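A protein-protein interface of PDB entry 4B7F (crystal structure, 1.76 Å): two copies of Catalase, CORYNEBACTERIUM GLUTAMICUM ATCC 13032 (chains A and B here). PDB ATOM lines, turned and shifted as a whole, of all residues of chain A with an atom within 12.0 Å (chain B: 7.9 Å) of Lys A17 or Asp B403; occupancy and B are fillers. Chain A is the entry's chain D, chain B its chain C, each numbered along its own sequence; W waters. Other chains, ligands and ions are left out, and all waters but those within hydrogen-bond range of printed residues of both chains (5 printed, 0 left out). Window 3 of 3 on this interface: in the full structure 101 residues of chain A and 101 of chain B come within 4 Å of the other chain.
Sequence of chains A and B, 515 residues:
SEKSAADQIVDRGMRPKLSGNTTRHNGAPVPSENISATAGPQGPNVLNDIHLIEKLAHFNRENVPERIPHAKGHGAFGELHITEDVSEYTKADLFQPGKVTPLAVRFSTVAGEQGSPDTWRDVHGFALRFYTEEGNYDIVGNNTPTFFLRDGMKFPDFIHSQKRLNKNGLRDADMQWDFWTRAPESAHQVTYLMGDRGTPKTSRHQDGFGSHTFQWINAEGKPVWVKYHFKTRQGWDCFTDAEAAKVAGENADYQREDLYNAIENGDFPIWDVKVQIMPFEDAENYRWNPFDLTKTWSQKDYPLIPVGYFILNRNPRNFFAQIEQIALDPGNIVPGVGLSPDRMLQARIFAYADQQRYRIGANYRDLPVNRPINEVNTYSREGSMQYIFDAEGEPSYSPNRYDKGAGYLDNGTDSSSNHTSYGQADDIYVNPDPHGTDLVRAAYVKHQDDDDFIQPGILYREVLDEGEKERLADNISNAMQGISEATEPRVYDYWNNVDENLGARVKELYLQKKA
ND2 of Asn B377 is in hydrogen-bond range of O of Asn A21 (3.0 Å).
N of Thr A23 is in hydrogen-bond range of O of Asn B377.
OD1 of Asp B390 lies within salt-bridge range of NH1 of Arg A15 (2.9 Å).
SD of Met A14 sits at hydrogen-bond distance from N of Glu B392 (3.5 Å).
OE1 of Glu B392 is in salt-bridge range of NH1 of Arg A317.
OD2 of Asp B403 is in salt-bridge range of NZ of Lys A17.
The backbone NH (N) of Thr A22 lies within hydrogen-bond range of the backbone carbonyl oxygen (O) of Ala B406, at 2.8 Å.
The side-chain amide oxygen (OD1) of Asn B377 sits at hydrogen-bond distance from the side-chain amino group (NZ) of Lys B404.
OH of Tyr B379 is in hydrogen-bond range of OD1 of Asn B400 (3.0 Å).
The side-chain hydroxyl of Tyr B379 is in hydrogen-bond range of the backbone carbonyl oxygen of Gly B405 (2.5 Å).
The side-chain amino group (NZ) of Lys B404 lies within salt-bridge range of the side-chain carboxylate (OD2) of Asp B390 (2.9 Å).
The guanidinium group of Arg A317 is in salt-bridge range of the side-chain carboxylate of Asp A11 (2.8 Å).
The side-chain carboxylate of Glu A33 lies within hydrogen-bond range of the side-chain hydroxyl of Thr A22 (2.7 Å).
CG of Met A14 touches O of Asp B390, at 3.7 Å.
Ala B391 touches Met A14 (CA to CG, 3.8 Å).
Ala B391 touches Arg A15 (CB to O, 3.6 Å).
Glu B394 touches Lys A17 (OE2 to CE, 3.1 Å).
Leu A18 touches Glu B375 (CD2 to CB, 3.8 Å).
Leu A18 touches Asn B377.
Leu A18 touches Lys B404.
CB of Ser A19 touches O of Asp B403, 3.5 Å away.
O of Lys B404 touches O of Gly A20, at 3.9 Å.
Thr A22 touches Tyr B379.
Lys A17 touches three residues of chain B.
Asp B403 touches two residues of chain A.
Ala B391 touches just these residues of chain A: Met A14 (3.8 Å), Arg A15 (3.6 Å) and Lys A17 (3.8 Å).
No residue of chain A comes within 4 Å of Asn B400.
Of chain A, only Gly A20 (3.5 Å) and Thr A22 (3.8 Å) come within 4 Å of Gly B405.
Of the printed residues of chain A, Glu B394 touches Lys A17 (3.1 Å).
Printed residues of chain B within 4 Å of Ser A19: Asp B403 (3.5 Å) and Lys B404 (3.7 Å).
Printed residues of chain B within 4 Å of Gly A20: Lys B404 and Gly B405.
Gly A13 touches none of the printed residues of chain B.
The nearest residue of chain B that does not touch Lys A17 is Lys B404 (5.3 Å).
The nearest residue of chain A that does not touch Asp B403 is Gly A20 (4.1 Å).
The nearest printed residue of chain B that does not touch Leu A18 is Glu B394 (4.2 Å).
Hydrophobic or aromatic side chains of chain A within 4 Å of the printed part of chain B: Met A14, Pro A16 and Leu A18.
Printed residues of chain B that touch a printed residue of chain A: Glu B375, Asn B377, Tyr B379, Asp B390, Ala B391, Glu B392, Glu B394, Asp B403, Lys B404, Gly B405 and Ala B406.
Among the printed residues, 25 pairs touch across the chains.
No position is printed for both chains.
Of the 25 pairs that touch across the chains among the printed residues, none has its exchanged pair printed and touching as well.
Water W4 lies within hydrogen-bond range of OE2 of Glu A33 (2.6 Å) and N of Tyr B379 (3.2 Å).
Water W3 lies within hydrogen-bond range of the backbone carbonyl oxygen (O) of Arg A317 (2.7 Å) and the backbone NH (N) of Gly B393 (3.0 Å).
Water W5 lies within hydrogen-bond range of O of Pro A16 (2.8 Å) and N of Ala B391 (3.0 Å).
Water W1 bridges OE2 of Glu B392 (2.8 Å) and NH1 of Arg A317 (3.2 Å).
Water W2 lies within hydrogen-bond range of the backbone NH (N) of Glu B392 (3.4 Å) and the side-chain sulfur (SD) of Met A14 (3.7 Å).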
ATOM      1  N   ASP A  11       0.419  -4.354  12.024  1.00  0.00           N
ATOM      2  CA  ASP A  11      -0.436  -3.346  11.399  1.00  0.00           C
ATOM      3  C   ASP A  11       0.123  -2.836  10.061  1.00  0.00           C
ATOM      4  O   ASP A  11      -0.593  -2.184   9.290  1.00  0.00           O
ATOM      5  CB  ASP A  11      -0.649  -2.164  12.348  1.00  0.00           C
ATOM      6  CG  ASP A  11      -1.650  -2.471  13.453  1.00  0.00           C
ATOM      7  OD1 ASP A  11      -2.309  -3.533  13.400  1.00  0.00           O
ATOM      8  OD2 ASP A  11      -1.782  -1.625  14.365  1.00  0.00           O
ATOM      9  N   GLY A  13       0.926  -2.405   6.377  1.00  0.00           N
ATOM     10  CA  GLY A  13       0.319  -2.843   5.131  1.00  0.00           C
ATOM     11  C   GLY A  13      -1.188  -2.999   5.162  1.00  0.00           C
ATOM     12  O   GLY A  13      -1.802  -3.274   4.133  1.00  0.00           O
ATOM     13  N   MET A  14      -1.798  -2.820   6.333  1.00  0.00           N
ATOM     14  CA  MET A  14      -3.226  -3.064   6.465  1.00  0.00           C
ATOM     15  C   MET A  14      -4.056  -1.837   6.082  1.00  0.00           C
ATOM     16  O   MET A  14      -3.815  -0.731   6.582  1.00  0.00           O
ATOM     17  CB  MET A  14      -3.577  -3.489   7.893  1.00  0.00           C
ATOM     18  CG  MET A  14      -5.047  -3.842   8.058  1.00  0.00           C
ATOM     19  SD  MET A  14      -5.392  -4.753   9.582  1.00  0.00           S
ATOM     20  CE  MET A  14      -4.712  -3.656  10.818  1.00  0.00           C
ATOM     21  N   ARG A  15      -5.027  -2.053   5.204  1.00  0.00           N
ATOM     22  CA  ARG A  15      -5.972  -1.016   4.791  1.00  0.00           C
ATOM     23  C   ARG A  15      -6.919  -0.649   5.924  1.00  0.00           C
ATOM     24  O   ARG A  15      -7.172  -1.470   6.820  1.00  0.00           O
ATOM     25  CB  ARG A  15      -6.832  -1.510   3.624  1.00  0.00           C
ATOM     26  CG  ARG A  15      -6.125  -1.701   2.297  1.00  0.00           C
ATOM     27  CD  ARG A  15      -7.161  -2.016   1.225  1.00  0.00           C
ATOM     28  NE  ARG A  15      -6.563  -2.068  -0.106  1.00  0.00           N
ATOM     29  CZ  ARG A  15      -6.254  -3.192  -0.743  1.00  0.00           C
ATOM     30  NH1 ARG A  15      -6.488  -4.368  -0.170  1.00  0.00           N
ATOM     31  NH2 ARG A  15      -5.707  -3.138  -1.953  1.00  0.00           N
ATOM     32  N   PRO A  16      -7.466   0.581   5.881  1.00  0.00           N
ATOM     33  CA  PRO A  16      -8.562   0.906   6.801  1.00  0.00           C
ATOM     34  C   PRO A  16      -9.779   0.111   6.369  1.00  0.00           C
ATOM     35  O   PRO A  16      -9.811  -0.396   5.232  1.00  0.00           O
ATOM     36  CB  PRO A  16      -8.812   2.392   6.528  1.00  0.00           C
ATOM     37  CG  PRO A  16      -8.427   2.566   5.080  1.00  0.00           C
ATOM     38  CD  PRO A  16      -7.212   1.670   4.916  1.00  0.00           C
ATOM     39  N   LYS A  17     -10.772  -0.007   7.244  1.00  0.00           N
ATOM     40  CA  LYS A  17     -12.006  -0.675   6.863  1.00  0.00           C
ATOM     41  C   LYS A  17     -12.735   0.207   5.852  1.00  0.00           C
ATOM     42  O   LYS A  17     -12.703   1.439   5.961  1.00  0.00           O
ATOM     43  CB  LYS A  17     -12.870  -0.932   8.094  1.00  0.00           C
ATOM     44  CG  LYS A  17     -14.055  -1.831   7.841  1.00  0.00           C
ATOM     45  CD  LYS A  17     -14.580  -2.387   9.158  1.00  0.00           C
ATOM     46  CE  LYS A  17     -15.919  -3.085   8.961  1.00  0.00           C
ATOM     47  NZ  LYS A  17     -16.916  -2.185   8.314  1.00  0.00           N
ATOM     48  N   LEU A  18     -13.357  -0.419   4.857  1.00  0.00           N
ATOM     49  CA  LEU A  18     -14.003   0.310   3.771  1.00  0.00           C
ATOM     50  C   LEU A  18     -15.442  -0.161   3.598  1.00  0.00           C
ATOM     51  O   LEU A  18     -15.778  -1.320   3.885  1.00  0.00           O
ATOM     52  CB  LEU A  18     -13.220   0.119   2.464  1.00  0.00           C
ATOM     53  CG  LEU A  18     -11.778   0.640   2.449  1.00  0.00           C
ATOM     54  CD1 LEU A  18     -11.061   0.243   1.153  1.00  0.00           C
ATOM     55  CD2 LEU A  18     -11.732   2.153   2.633  1.00  0.00           C
ATOM     56  N   SER A  19     -16.299   0.745   3.139  1.00  0.00           N
ATOM     57  CA  SER A  19     -17.691   0.405   2.884  1.00  0.00           C
ATOM     58  C   SER A  19     -18.195   1.166   1.667  1.00  0.00           C
ATOM     59  O   SER A  19     -17.427   1.844   0.984  1.00  0.00           O
ATOM     60  CB  SER A  19     -18.561   0.730   4.101  1.00  0.00           C
ATOM     61  OG  SER A  19     -18.536   2.122   4.377  1.00  0.00           O
ATOM     62  N   GLY A  20     -19.488   1.057   1.397  1.00  0.00           N
ATOM     63  CA  GLY A  20     -20.041   1.691   0.220  1.00  0.00           C
ATOM     64  C   GLY A  20     -20.017   0.681  -0.905  1.00  0.00           C
ATOM     65  O   GLY A  20     -20.647  -0.372  -0.804  1.00  0.00           O
ATOM     66  N   ASN A  21     -19.290   0.982  -1.975  1.00  0.00           N
ATOM     67  CA  ASN A  21     -19.224   0.061  -3.094  1.00  0.00           C
ATOM     68  C   ASN A  21     -17.792  -0.313  -3.394  1.00  0.00           C
ATOM     69  O   ASN A  21     -16.853   0.318  -2.906  1.00  0.00           O
ATOM     70  CB  ASN A  21     -19.844   0.669  -4.355  1.00  0.00           C
ATOM     71  CG  ASN A  21     -20.753   1.826  -4.053  1.00  0.00           C
ATOM     72  OD1 ASN A  21     -20.376   2.985  -4.237  1.00  0.00           O
ATOM     73  ND2 ASN A  21     -21.959   1.526  -3.578  1.00  0.00           N
ATOM     74  N   THR A  22     -17.622  -1.327  -4.229  1.00  0.00           N
ATOM     75  CA  THR A  22     -16.281  -1.775  -4.560  1.00  0.00           C
ATOM     76  C   THR A  22     -15.697  -0.903  -5.662  1.00  0.00           C
ATOM     77  O   THR A  22     -16.435  -0.190  -6.351  1.00  0.00           O
ATOM     78  CB  THR A  22     -16.284  -3.254  -4.970  1.00  0.00           C
ATOM     79  OG1 THR A  22     -17.333  -3.492  -5.923  1.00  0.00           O
ATOM     80  CG2 THR A  22     -16.522  -4.130  -3.738  1.00  0.00           C
ATOM     81  N   THR A  23     -14.375  -0.933  -5.797  1.00  0.00           N
ATOM     82  CA  THR A  23     -13.698  -0.240  -6.889  1.00  0.00           C
ATOM     83  C   THR A  23     -12.832  -1.225  -7.664  1.00  0.00           C
ATOM     84  O   THR A  23     -12.444  -2.270  -7.128  1.00  0.00           O
ATOM     85  CB  THR A  23     -12.760   0.907  -6.389  1.00  0.00           C
ATOM     86  OG1 THR A  23     -11.590   0.352  -5.774  1.00  0.00           O
ATOM     87  CG2 THR A  23     -13.460   1.831  -5.410  1.00  0.00           C
ATOM     88  N   GLU A  33     -20.841  -6.795  -8.980  1.00  0.00           N
ATOM     89  CA  GLU A  33     -20.080  -7.987  -8.605  1.00  0.00           C
ATOM     90  C   GLU A  33     -20.897  -9.231  -8.944  1.00  0.00           C
ATOM     91  O   GLU A  33     -20.502 -10.357  -8.616  1.00  0.00           O
ATOM     92  CB  GLU A  33     -19.785  -7.999  -7.096  1.00  0.00           C
ATOM     93  CG  GLU A  33     -18.936  -6.840  -6.562  1.00  0.00           C
ATOM     94  CD  GLU A  33     -17.481  -6.911  -6.995  1.00  0.00           C
ATOM     95  OE1 GLU A  33     -17.128  -7.824  -7.777  1.00  0.00           O
ATOM     96  OE2 GLU A  33     -16.683  -6.048  -6.551  1.00  0.00           O
ATOM     97  N   ARG A 317      -3.236 -10.344  11.423  1.00  0.00           N
ATOM     98  CA  ARG A 317      -4.330  -9.602  10.798  1.00  0.00           C
ATOM     99  C   ARG A 317      -4.785 -10.309   9.527  1.00  0.00           C
ATOM    100  O   ARG A 317      -5.980 -10.382   9.228  1.00  0.00           O
ATOM    101  CB  ARG A 317      -3.897  -8.180  10.436  1.00  0.00           C
ATOM    102  CG  ARG A 317      -3.234  -7.400  11.556  1.00  0.00           C
ATOM    103  CD  ARG A 317      -4.170  -7.192  12.725  1.00  0.00           C
ATOM    104  NE  ARG A 317      -3.723  -6.075  13.550  1.00  0.00           N
ATOM    105  CZ  ARG A 317      -4.065  -5.894  14.820  1.00  0.00           C
ATOM    106  NH1 ARG A 317      -4.854  -6.767  15.430  1.00  0.00           N
ATOM    107  NH2 ARG A 317      -3.607  -4.841  15.483  1.00  0.00           N
ATOM    108  N   GLU B 375      -8.722   4.997  -1.731  1.00  0.00           N
ATOM    109  CA  GLU B 375      -8.592   3.611  -1.291  1.00  0.00           C
ATOM    110  C   GLU B 375      -9.234   2.675  -2.307  1.00  0.00           C
ATOM    111  O   GLU B 375     -10.314   2.958  -2.804  1.00  0.00           O
ATOM    112  CB  GLU B 375      -9.284   3.411   0.061  1.00  0.00           C
ATOM    113  CG  GLU B 375      -8.570   4.052   1.238  1.00  0.00           C
ATOM    114  CD  GLU B 375      -7.234   3.401   1.532  1.00  0.00           C
ATOM    115  OE1 GLU B 375      -6.999   2.265   1.065  1.00  0.00           O
ATOM    116  OE2 GLU B 375      -6.415   4.027   2.233  1.00  0.00           O
ATOM    117  N   ASN B 377     -11.212  -0.666  -2.877  1.00  0.00           N
ATOM    118  CA  ASN B 377     -12.095  -1.563  -2.142  1.00  0.00           C
ATOM    119  C   ASN B 377     -12.354  -2.768  -3.021  1.00  0.00           C
ATOM    120  O   ASN B 377     -13.254  -2.740  -3.866  1.00  0.00           O
ATOM    121  CB  ASN B 377     -13.429  -0.867  -1.830  1.00  0.00           C
ATOM    122  CG  ASN B 377     -14.295  -1.662  -0.873  1.00  0.00           C
ATOM    123  OD1 ASN B 377     -13.810  -2.585  -0.215  1.00  0.00           O
ATOM    124  ND2 ASN B 377     -15.588  -1.316  -0.796  1.00  0.00           N
ATOM    125  N   TYR B 379     -12.269  -7.311  -3.657  1.00  0.00           N
ATOM    126  CA  TYR B 379     -12.299  -8.643  -3.065  1.00  0.00           C
ATOM    127  C   TYR B 379     -11.127  -9.494  -3.535  1.00  0.00           C
ATOM    128  O   TYR B 379     -10.946 -10.605  -3.041  1.00  0.00           O
ATOM    129  CB  TYR B 379     -13.634  -9.347  -3.335  1.00  0.00           C
ATOM    130  CG  TYR B 379     -14.756  -8.789  -2.489  1.00  0.00           C
ATOM    131  CD1 TYR B 379     -14.932  -9.205  -1.175  1.00  0.00           C
ATOM    132  CD2 TYR B 379     -15.619  -7.825  -2.994  1.00  0.00           C
ATOM    133  CE1 TYR B 379     -15.958  -8.682  -0.384  1.00  0.00           C
ATOM    134  CE2 TYR B 379     -16.640  -7.298  -2.218  1.00  0.00           C
ATOM    135  CZ  TYR B 379     -16.809  -7.733  -0.919  1.00  0.00           C
ATOM    136  OH  TYR B 379     -17.818  -7.202  -0.147  1.00  0.00           O
ATOM    137  N   ASP B 390      -6.502  -6.132   3.217  1.00  0.00           N
ATOM    138  CA  ASP B 390      -7.700  -5.526   3.810  1.00  0.00           C
ATOM    139  C   ASP B 390      -7.682  -5.521   5.341  1.00  0.00           C
ATOM    140  O   ASP B 390      -6.932  -6.266   5.967  1.00  0.00           O
ATOM    141  CB  ASP B 390      -8.956  -6.264   3.357  1.00  0.00           C
ATOM    142  CG  ASP B 390      -9.486  -5.770   2.027  1.00  0.00           C
ATOM    143  OD1 ASP B 390      -8.866  -4.869   1.417  1.00  0.00           O
ATOM    144  OD2 ASP B 390     -10.523  -6.307   1.581  1.00  0.00           O
ATOM    145  N   ALA B 391      -8.536  -4.690   5.935  1.00  0.00           N
ATOM    146  CA  ALA B 391      -8.679  -4.649   7.391  1.00  0.00           C
ATOM    147  C   ALA B 391      -8.994  -6.041   7.933  1.00  0.00           C
ATOM    148  O   ALA B 391      -9.694  -6.818   7.289  1.00  0.00           O
ATOM    149  CB  ALA B 391      -9.785  -3.680   7.785  1.00  0.00           C
ATOM    150  N   GLU B 392      -8.485  -6.343   9.120  1.00  0.00           N
ATOM    151  CA  GLU B 392      -8.618  -7.681   9.690  1.00  0.00           C
ATOM    152  C   GLU B 392     -10.046  -8.241   9.675  1.00  0.00           C
ATOM    153  O   GLU B 392     -10.990  -7.601  10.145  1.00  0.00           O
ATOM    154  CB  GLU B 392      -8.054  -7.680  11.110  1.00  0.00           C
ATOM    155  CG  GLU B 392      -8.260  -8.980  11.870  1.00  0.00           C
ATOM    156  CD  GLU B 392      -7.673  -8.918  13.258  1.00  0.00           C
ATOM    157  OE1 GLU B 392      -7.430  -7.789  13.749  1.00  0.00           O
ATOM    158  OE2 GLU B 392      -7.439  -9.990  13.856  1.00  0.00           O
ATOM    159  N   GLY B 393     -10.211  -9.430   9.102  1.00  0.00           N
ATOM    160  CA  GLY B 393     -11.483 -10.125   9.183  1.00  0.00           C
ATOM    161  C   GLY B 393     -12.533  -9.704   8.176  1.00  0.00           C
ATOM    162  O   GLY B 393     -13.636 -10.244   8.178  1.00  0.00           O
ATOM    163  N   GLU B 394     -12.206  -8.749   7.305  1.00  0.00           N
ATOM    164  CA  GLU B 394     -13.156  -8.322   6.273  1.00  0.00           C
ATOM    165  C   GLU B 394     -13.496  -9.510   5.366  1.00  0.00           C
ATOM    166  O   GLU B 394     -12.662 -10.403   5.177  1.00  0.00           O
ATOM    167  CB  GLU B 394     -12.585  -7.152   5.458  1.00  0.00           C
ATOM    168  CG  GLU B 394     -12.551  -5.832   6.220  1.00  0.00           C
ATOM    169  CD  GLU B 394     -13.933  -5.367   6.621  1.00  0.00           C
ATOM    170  OE1 GLU B 394     -14.674  -4.876   5.741  1.00  0.00           O
ATOM    171  OE2 GLU B 394     -14.285  -5.510   7.813  1.00  0.00           O
ATOM    172  N   PRO B 395     -14.730  -9.550   4.832  1.00  0.00           N
ATOM    173  CA  PRO B 395     -15.139 -10.692   4.002  1.00  0.00           C
ATOM    174  C   PRO B 395     -14.387 -10.767   2.674  1.00  0.00           C
ATOM    175  O   PRO B 395     -13.960  -9.739   2.132  1.00  0.00           O
ATOM    176  CB  PRO B 395     -16.618 -10.416   3.735  1.00  0.00           C
ATOM    177  CG  PRO B 395     -16.736  -8.902   3.855  1.00  0.00           C
ATOM    178  CD  PRO B 395     -15.819  -8.568   4.994  1.00  0.00           C
ATOM    179  N   ASN B 400     -22.361 -10.531   1.000  1.00  0.00           N
ATOM    180  CA  ASN B 400     -22.114 -11.002   2.358  1.00  0.00           C
ATOM    181  C   ASN B 400     -22.967 -10.229   3.363  1.00  0.00           C
ATOM    182  O   ASN B 400     -23.661  -9.281   2.990  1.00  0.00           O
ATOM    183  CB  ASN B 400     -20.630 -10.883   2.709  1.00  0.00           C
ATOM    184  CG  ASN B 400     -20.084  -9.482   2.497  1.00  0.00           C
ATOM    185  OD1 ASN B 400     -19.400  -9.205   1.504  1.00  0.00           O
ATOM    186  ND2 ASN B 400     -20.363  -8.593   3.436  1.00  0.00           N
ATOM    187  N   ARG B 401     -22.893 -10.615   4.633  1.00  0.00           N
ATOM    188  CA  ARG B 401     -23.735 -10.011   5.667  1.00  0.00           C
ATOM    189  C   ARG B 401     -23.045  -8.869   6.396  1.00  0.00           C
ATOM    190  O   ARG B 401     -23.516  -8.425   7.445  1.00  0.00           O
ATOM    191  CB  ARG B 401     -24.183 -11.082   6.675  1.00  0.00           C
ATOM    192  CG  ARG B 401     -23.047 -11.724   7.480  1.00  0.00           C
ATOM    193  CD  ARG B 401     -23.596 -12.859   8.343  1.00  0.00           C
ATOM    194  NE  ARG B 401     -22.564 -13.546   9.118  1.00  0.00           N
ATOM    195  CZ  ARG B 401     -22.242 -13.242  10.373  1.00  0.00           C
ATOM    196  NH1 ARG B 401     -22.856 -12.244  10.995  1.00  0.00           N
ATOM    197  NH2 ARG B 401     -21.299 -13.926  11.003  1.00  0.00           N
ATOM    198  N   TYR B 402     -21.939  -8.385   5.834  1.00  0.00           N
ATOM    199  CA  TYR B 402     -21.157  -7.329   6.469  1.00  0.00           C
ATOM    200  C   TYR B 402     -21.220  -6.016   5.669  1.00  0.00           C
ATOM    201  O   TYR B 402     -22.132  -5.828   4.866  1.00  0.00           O
ATOM    202  CB  TYR B 402     -19.714  -7.795   6.673  1.00  0.00           C
ATOM    203  CG  TYR B 402     -19.603  -9.170   7.309  1.00  0.00           C
ATOM    204  CD1 TYR B 402     -19.910  -9.369   8.654  1.00  0.00           C
ATOM    205  CD2 TYR B 402     -19.172 -10.269   6.566  1.00  0.00           C
ATOM    206  CE1 TYR B 402     -19.799 -10.628   9.236  1.00  0.00           C
ATOM    207  CE2 TYR B 402     -19.060 -11.528   7.140  1.00  0.00           C
ATOM    208  CZ  TYR B 402     -19.374 -11.700   8.472  1.00  0.00           C
ATOM    209  OH  TYR B 402     -19.270 -12.946   9.048  1.00  0.00           O
ATOM    210  N   ASP B 403     -20.257  -5.123   5.882  1.00  0.00           N
ATOM    211  CA  ASP B 403     -20.341  -3.748   5.361  1.00  0.00           C
ATOM    212  C   ASP B 403     -19.547  -3.454   4.089  1.00  0.00           C
ATOM    213  O   ASP B 403     -19.783  -2.432   3.433  1.00  0.00           O
ATOM    214  CB  ASP B 403     -19.848  -2.754   6.415  1.00  0.00           C
ATOM    215  CG  ASP B 403     -20.824  -2.556   7.542  1.00  0.00           C
ATOM    216  OD1 ASP B 403     -21.933  -3.124   7.485  1.00  0.00           O
ATOM    217  OD2 ASP B 403     -20.470  -1.813   8.482  1.00  0.00           O
ATOM    218  N   LYS B 404     -18.579  -4.308   3.769  1.00  0.00           N
ATOM    219  CA  LYS B 404     -17.626  -4.020   2.689  1.00  0.00           C
ATOM    220  C   LYS B 404     -18.277  -3.586   1.374  1.00  0.00           C
ATOM    221  O   LYS B 404     -17.820  -2.630   0.731  1.00  0.00           O
ATOM    222  CB  LYS B 404     -16.705  -5.218   2.455  1.00  0.00           C
ATOM    223  CG  LYS B 404     -15.580  -4.962   1.466  1.00  0.00           C
ATOM    224  CD  LYS B 404     -14.572  -6.104   1.531  1.00  0.00           C
ATOM    225  CE  LYS B 404     -13.677  -6.144   0.298  1.00  0.00           C
ATOM    226  NZ  LYS B 404     -12.727  -5.003   0.295  1.00  0.00           N
ATOM    227  N   GLY B 405     -19.333  -4.279   0.969  1.00  0.00           N
ATOM    228  CA  GLY B 405     -20.141  -3.791  -0.129  1.00  0.00           C
ATOM    229  C   GLY B 405     -19.942  -4.550  -1.420  1.00  0.00           C
ATOM    230  O   GLY B 405     -19.199  -5.536  -1.475  1.00  0.00           O
ATOM    231  N   ALA B 406     -20.616  -4.079  -2.467  1.00  0.00           N
ATOM    232  CA  ALA B 406     -20.539  -4.694  -3.782  1.00  0.00           C
ATOM    233  C   ALA B 406     -20.607  -3.594  -4.837  1.00  0.00           C
ATOM    234  O   ALA B 406     -20.209  -2.469  -4.573  1.00  0.00           O
ATOM    235  CB  ALA B 406     -21.670  -5.693  -3.959  1.00  0.00           C
ATOM    236  N   GLY B 412     -26.029  -4.957  -2.515  1.00  0.00           N
ATOM    237  CA  GLY B 412     -25.095  -5.243  -1.443  1.00  0.00           C
ATOM    238  C   GLY B 412     -25.492  -6.404  -0.543  1.00  0.00           C
ATOM    239  O   GLY B 412     -24.750  -6.755   0.378  1.00  0.00           O
HETATM  240  O   HOH W   1      -5.105  -9.923  15.331  1.00  0.00           O
HETATM  241  O   HOH W   2      -8.573  -3.601  11.162  1.00  0.00           O
HETATM  242  O   HOH W   3      -8.016 -10.600   7.395  1.00  0.00           O
HETATM  243  O   HOH W   4     -14.128  -6.263  -6.053  1.00  0.00           O
HETATM  244  O   HOH W   5     -10.067  -2.877   4.050  1.00  0.00           O
